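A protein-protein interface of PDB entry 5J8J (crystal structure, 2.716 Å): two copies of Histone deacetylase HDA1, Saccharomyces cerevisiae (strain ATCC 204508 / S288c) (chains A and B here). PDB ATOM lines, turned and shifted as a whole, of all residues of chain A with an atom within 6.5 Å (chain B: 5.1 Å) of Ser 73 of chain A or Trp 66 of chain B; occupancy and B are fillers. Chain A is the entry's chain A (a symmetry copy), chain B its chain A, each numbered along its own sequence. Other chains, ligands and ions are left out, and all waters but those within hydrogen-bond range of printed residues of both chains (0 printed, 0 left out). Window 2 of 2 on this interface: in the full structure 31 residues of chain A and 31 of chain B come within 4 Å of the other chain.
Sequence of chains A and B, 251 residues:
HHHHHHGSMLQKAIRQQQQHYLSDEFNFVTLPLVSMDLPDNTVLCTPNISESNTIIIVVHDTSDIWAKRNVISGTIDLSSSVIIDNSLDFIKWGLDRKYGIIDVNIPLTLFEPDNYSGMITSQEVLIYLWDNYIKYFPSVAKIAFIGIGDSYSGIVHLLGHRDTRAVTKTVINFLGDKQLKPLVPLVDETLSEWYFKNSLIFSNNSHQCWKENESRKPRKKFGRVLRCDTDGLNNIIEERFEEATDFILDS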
ATOM      1  N   HIS A   3      -4.155 -15.587 -23.282  1.00  0.00           N
ATOM      2  CA  HIS A   3      -2.980 -16.420 -22.990  1.00  0.00           C
ATOM      3  C   HIS A   3      -3.341 -17.866 -22.652  1.00  0.00           C
ATOM      4  O   HIS A   3      -4.050 -18.131 -21.695  1.00  0.00           O
ATOM      5  CB  HIS A   3      -2.156 -15.834 -21.840  1.00  0.00           C
ATOM      6  CG  HIS A   3      -1.398 -14.600 -22.206  1.00  0.00           C
ATOM      7  ND1 HIS A   3      -0.838 -13.759 -21.270  1.00  0.00           N
ATOM      8  CD2 HIS A   3      -1.093 -14.066 -23.417  1.00  0.00           C
ATOM      9  CE1 HIS A   3      -0.244 -12.747 -21.881  1.00  0.00           C
ATOM     10  NE2 HIS A   3      -0.381 -12.916 -23.185  1.00  0.00           N
ATOM     11  N   ARG A  69      12.310 -16.249 -11.097  1.00  0.00           N
ATOM     12  CA  ARG A  69      11.373 -15.556 -11.945  1.00  0.00           C
ATOM     13  C   ARG A  69      11.628 -14.071 -12.090  1.00  0.00           C
ATOM     14  O   ARG A  69      11.442 -13.309 -11.159  1.00  0.00           O
ATOM     15  CB  ARG A  69       9.940 -15.854 -11.468  1.00  0.00           C
ATOM     16  CG  ARG A  69       9.081 -14.694 -10.991  1.00  0.00           C
ATOM     17  CD  ARG A  69       7.610 -15.013 -11.184  1.00  0.00           C
ATOM     18  NE  ARG A  69       6.727 -14.064 -10.518  1.00  0.00           N
ATOM     19  CZ  ARG A  69       5.428 -13.954 -10.767  1.00  0.00           C
ATOM     20  N   ASN A  70      12.046 -13.674 -13.280  1.00  0.00           N
ATOM     21  CA  ASN A  70      12.291 -12.258 -13.581  1.00  0.00           C
ATOM     22  C   ASN A  70      11.116 -11.498 -12.977  1.00  0.00           C
ATOM     23  O   ASN A  70       9.979 -11.639 -13.425  1.00  0.00           O
ATOM     24  CB  ASN A  70      12.436 -12.013 -15.097  1.00  0.00           C
ATOM     25  CG  ASN A  70      12.574 -10.516 -15.472  1.00  0.00           C
ATOM     26  OD1 ASN A  70      11.896  -9.638 -14.928  1.00  0.00           O
ATOM     27  ND2 ASN A  70      13.458 -10.235 -16.428  1.00  0.00           N
ATOM     28  N   VAL A  71      11.403 -10.726 -11.930  1.00  0.00           N
ATOM     29  CA  VAL A  71      10.375 -10.226 -11.016  1.00  0.00           C
ATOM     30  C   VAL A  71       9.316  -9.326 -11.674  1.00  0.00           C
ATOM     31  O   VAL A  71       8.136  -9.407 -11.321  1.00  0.00           O
ATOM     32  CB  VAL A  71      11.019  -9.456  -9.821  1.00  0.00           C
ATOM     33  CG1 VAL A  71      11.631  -8.113 -10.271  1.00  0.00           C
ATOM     34  CG2 VAL A  71       9.997  -9.258  -8.692  1.00  0.00           C
ATOM     35  N   ILE A  72       9.716  -8.489 -12.632  1.00  0.00           N
ATOM     36  CA  ILE A  72       8.780  -7.523 -13.198  1.00  0.00           C
ATOM     37  C   ILE A  72       8.097  -8.041 -14.468  1.00  0.00           C
ATOM     38  O   ILE A  72       6.934  -7.714 -14.722  1.00  0.00           O
ATOM     39  CB  ILE A  72       9.468  -6.165 -13.484  1.00  0.00           C
ATOM     40  CG1 ILE A  72       8.412  -5.094 -13.774  1.00  0.00           C
ATOM     41  CG2 ILE A  72      10.491  -6.280 -14.615  1.00  0.00           C
ATOM     42  CD1 ILE A  72       7.320  -5.009 -12.711  1.00  0.00           C
ATOM     43  N   SER A  73       8.799  -8.854 -15.256  1.00  0.00           N
ATOM     44  CA  SER A  73       8.165  -9.480 -16.410  1.00  0.00           C
ATOM     45  C   SER A  73       7.294 -10.613 -15.899  1.00  0.00           C
ATOM     46  O   SER A  73       6.271 -10.948 -16.495  1.00  0.00           O
ATOM     47  CB  SER A  73       9.194 -10.000 -17.410  1.00  0.00           C
ATOM     48  OG  SER A  73       9.916 -11.082 -16.863  1.00  0.00           O
ATOM     49  N   GLY A  74       7.710 -11.193 -14.776  1.00  0.00           N
ATOM     50  CA  GLY A  74       6.938 -12.220 -14.101  1.00  0.00           C
ATOM     51  C   GLY A  74       7.106 -13.583 -14.733  1.00  0.00           C
ATOM     52  O   GLY A  74       6.435 -14.539 -14.351  1.00  0.00           O
ATOM     53  N   THR A  75       8.002 -13.674 -15.707  1.00  0.00           N
ATOM     54  CA  THR A  75       8.172 -14.911 -16.452  1.00  0.00           C
ATOM     55  C   THR A  75       9.253 -15.763 -15.824  1.00  0.00           C
ATOM     56  O   THR A  75      10.121 -15.263 -15.120  1.00  0.00           O
ATOM     57  CB  THR A  75       8.517 -14.650 -17.934  1.00  0.00           C
ATOM     58  OG1 THR A  75       9.642 -13.767 -18.014  1.00  0.00           O
ATOM     59  CG2 THR A  75       7.336 -14.032 -18.663  1.00  0.00           C
ATOM     60  N   ILE A  76       9.190 -17.054 -16.109  1.00  0.00           N
ATOM     61  CA  ILE A  76      10.020 -18.051 -15.461  1.00  0.00           C
ATOM     62  C   ILE A  76      11.377 -18.224 -16.150  1.00  0.00           C
ATOM     63  O   ILE A  76      11.443 -18.432 -17.357  1.00  0.00           O
ATOM     64  CB  ILE A  76       9.259 -19.403 -15.416  1.00  0.00           C
ATOM     65  CG1 ILE A  76       8.342 -19.466 -14.190  1.00  0.00           C
ATOM     66  CG2 ILE A  76      10.226 -20.580 -15.391  1.00  0.00           C
ATOM     67  CD1 ILE A  76       7.230 -18.430 -14.125  1.00  0.00           C
ATOM     68  N   ASP B  64       7.993 -17.334 -23.757  1.00  0.00           N
ATOM     69  CA  ASP B  64       8.037 -17.297 -22.296  1.00  0.00           C
ATOM     70  C   ASP B  64       6.842 -18.031 -21.700  1.00  0.00           C
ATOM     71  O   ASP B  64       5.814 -18.225 -22.350  1.00  0.00           O
ATOM     72  CB  ASP B  64       8.044 -15.859 -21.760  1.00  0.00           C
ATOM     73  CG  ASP B  64       9.398 -15.172 -21.878  1.00  0.00           C
ATOM     74  OD1 ASP B  64      10.386 -15.826 -22.250  1.00  0.00           O
ATOM     75  OD2 ASP B  64       9.473 -13.962 -21.573  1.00  0.00           O
ATOM     76  N   ILE B  65       7.003 -18.432 -20.446  1.00  0.00           N
ATOM     77  CA  ILE B  65       5.933 -18.957 -19.629  1.00  0.00           C
ATOM     78  C   ILE B  65       5.781 -18.026 -18.458  1.00  0.00           C
ATOM     79  O   ILE B  65       6.748 -17.719 -17.767  1.00  0.00           O
ATOM     80  CB  ILE B  65       6.225 -20.369 -19.109  1.00  0.00           C
ATOM     81  CG1 ILE B  65       6.396 -21.343 -20.265  1.00  0.00           C
ATOM     82  CG2 ILE B  65       5.114 -20.846 -18.168  1.00  0.00           C
ATOM     83  CD1 ILE B  65       6.743 -22.707 -19.791  1.00  0.00           C
ATOM     84  N   TRP B  66       4.565 -17.552 -18.251  1.00  0.00           N
ATOM     85  CA  TRP B  66       4.274 -16.759 -17.083  1.00  0.00           C
ATOM     86  C   TRP B  66       3.509 -17.642 -16.129  1.00  0.00           C
ATOM     87  O   TRP B  66       2.637 -18.415 -16.535  1.00  0.00           O
ATOM     88  CB  TRP B  66       3.471 -15.509 -17.440  1.00  0.00           C
ATOM     89  CG  TRP B  66       3.245 -14.606 -16.274  1.00  0.00           C
ATOM     90  CD1 TRP B  66       4.012 -13.539 -15.904  1.00  0.00           C
ATOM     91  CD2 TRP B  66       2.187 -14.694 -15.311  1.00  0.00           C
ATOM     92  NE1 TRP B  66       3.495 -12.957 -14.774  1.00  0.00           N
ATOM     93  CE2 TRP B  66       2.375 -13.649 -14.389  1.00  0.00           C
ATOM     94  CE3 TRP B  66       1.099 -15.558 -15.139  1.00  0.00           C
ATOM     95  CZ2 TRP B  66       1.520 -13.445 -13.308  1.00  0.00           C
ATOM     96  CZ3 TRP B  66       0.248 -15.351 -14.067  1.00  0.00           C
ATOM     97  CH2 TRP B  66       0.465 -14.305 -13.166  1.00  0.00           C
ATOM     98  N   ALA B  67       3.838 -17.531 -14.855  1.00  0.00           N
ATOM     99  CA  ALA B  67       3.100 -18.246 -13.842  1.00  0.00           C
ATOM    100  C   ALA B  67       3.314 -17.547 -12.524  1.00  0.00           C
ATOM    101  O   ALA B  67       4.395 -17.013 -12.284  1.00  0.00           O
ATOM    102  CB  ALA B  67       3.556 -19.692 -13.769  1.00  0.00           C
ATOM    103  N   LYS B  68       2.298 -17.534 -11.670  1.00  0.00           N
ATOM    104  CA  LYS B  68       2.519 -17.081 -10.308  1.00  0.00           C
ATOM    105  C   LYS B  68       3.415 -18.081  -9.596  1.00  0.00           C
ATOM    106  O   LYS B  68       3.661 -19.194 -10.071  1.00  0.00           O
ATOM    107  CB  LYS B  68       1.211 -16.894  -9.525  1.00  0.00           C
ATOM    108  N   SER B  80      -1.709 -21.678 -12.794  1.00  0.00           N
ATOM    109  CA  SER B  80      -1.584 -20.300 -13.264  1.00  0.00           C
ATOM    110  C   SER B  80      -0.642 -20.154 -14.457  1.00  0.00           C
ATOM    111  O   SER B  80      -0.489 -19.070 -15.000  1.00  0.00           O
ATOM    112  CB  SER B  80      -1.083 -19.406 -12.145  1.00  0.00           C
ATOM    113  OG  SER B  80       0.334 -19.377 -12.134  1.00  0.00           O
ATOM    114  N   SER B  81       0.013 -21.236 -14.852  1.00  0.00           N
ATOM    115  CA  SER B  81       1.024 -21.142 -15.896  1.00  0.00           C
ATOM    116  C   SER B  81       0.393 -20.975 -17.272  1.00  0.00           C
ATOM    117  O   SER B  81      -0.561 -21.673 -17.617  1.00  0.00           O
ATOM    118  CB  SER B  81       1.932 -22.372 -15.868  1.00  0.00           C
ATOM    119  OG  SER B  81       1.181 -23.554 -16.026  1.00  0.00           O
ATOM    120  N   VAL B  82       0.929 -20.041 -18.048  1.00  0.00           N
ATOM    121  CA  VAL B  82       0.401 -19.735 -19.381  1.00  0.00           C
ATOM    122  C   VAL B  82       1.536 -19.425 -20.327  1.00  0.00           C
ATOM    123  O   VAL B  82       2.607 -18.990 -19.898  1.00  0.00           O
ATOM    124  CB  VAL B  82      -0.583 -18.520 -19.386  1.00  0.00           C
ATOM    125  CG1 VAL B  82      -1.907 -18.889 -18.751  1.00  0.00           C
ATOM    126  CG2 VAL B  82       0.033 -17.322 -18.685  1.00  0.00           C
ATOM    127  N   ILE B  84       3.105 -17.088 -23.073  1.00  0.00           N
ATOM    128  CA  ILE B  84       3.074 -15.756 -23.665  1.00  0.00           C
ATOM    129  C   ILE B  84       3.601 -15.848 -25.097  1.00  0.00           C
ATOM    130  O   ILE B  84       4.798 -15.715 -25.358  1.00  0.00           O
ATOM    131  CB  ILE B  84       3.889 -14.755 -22.823  1.00  0.00           C
ATOM    132  CG1 ILE B  84       3.329 -14.724 -21.397  1.00  0.00           C
ATOM    133  CG2 ILE B  84       3.862 -13.359 -23.437  1.00  0.00           C
ATOM    134  CD1 ILE B  84       3.885 -13.623 -20.559  1.00  0.00           C
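The backbone carbonyl oxygen of Ile 65 of chain B is in hydrogen-bond range of the backbone NH of Ile 76 of chain A, at 3.0 Å. NE1 of Trp 66 of chain B sits close to O of Gly 74 of chain A (3.4 Å).
N of Ile 84 of chain B sits at hydrogen-bond distance from O of Asp 64 of chain B (3.0 Å). O of Trp 66 of chain B lies within hydrogen-bond range of N of Val 82 of chain B (2.8 Å). The side-chain amide oxygen of Asn 70 of chain A lies close to the side-chain hydroxyl of Ser 73 of chain A (3.1 Å). The backbone NH of Asn 70 of chain A lies within hydrogen-bond range of the backbone carbonyl oxygen of Thr 75 of chain A, 3.1 Å away. The side-chain hydroxyl (OG1) of Thr 75 of chain A lies within hydrogen-bond range of the side-chain hydroxyl (OG) of Ser 73 of chain A, 2.9 Å away.
Along chain B the printed residues that touch a printed residue of chain A span positions 64 to 84. Hydrophobic or aromatic side chains of chain A within 4 Å of the printed part of chain B: His 3 and Ile 76.
Asn 70 of chain A touches none of the printed residues of chain B. Ile 72 of chain A touches none of the printed residues of chain B. Of chain B, only Trp 66 (3.5 Å) comes within 4 Å of Ser 73 of chain A. Of the printed residues of chain B, Thr 75 of chain A touches Asp 64, Ile 65, Trp 66 and Ile 84. Of the printed residues of chain A, Trp 66 of chain B touches Ser 73, Gly 74 and Thr 75. Of the printed residues of chain A, Ala 67 of chain B touches Arg 69, Gly 74 and Ile 76. The nearest printed residue of chain B that does not touch Ser 73 of chain A is Ile 84 of chain B (5.4 Å). The nearest printed residue of chain A that does not touch Trp 66 of chain B is Ile 76 of chain A (4.3 Å).
Among the printed residues, pairs that only touch across the chains: Thr 75 of chain A with Ile 65 of chain B (3.4 Å), Ser 73 of chain A with Trp 66 of chain B (3.5 Å), Arg 69 of chain A with Ala 67 of chain B (3.6 Å), Thr 75 of chain A with Asp 64 of chain B (3.6 Å), Ile 76 of chain A with Ala 67 of chain B (3.6 Å), His 3 of chain A with Val 82 of chain B (3.7 Å), Gly 74 of chain A with Ala 67 of chain B (3.8 Å), Thr 75 of chain A with Ile 84 of chain B (3.96 Å) and Thr 75 of chain A with Trp 66 of chain B (3.997 Å).
No position is printed for both chains.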
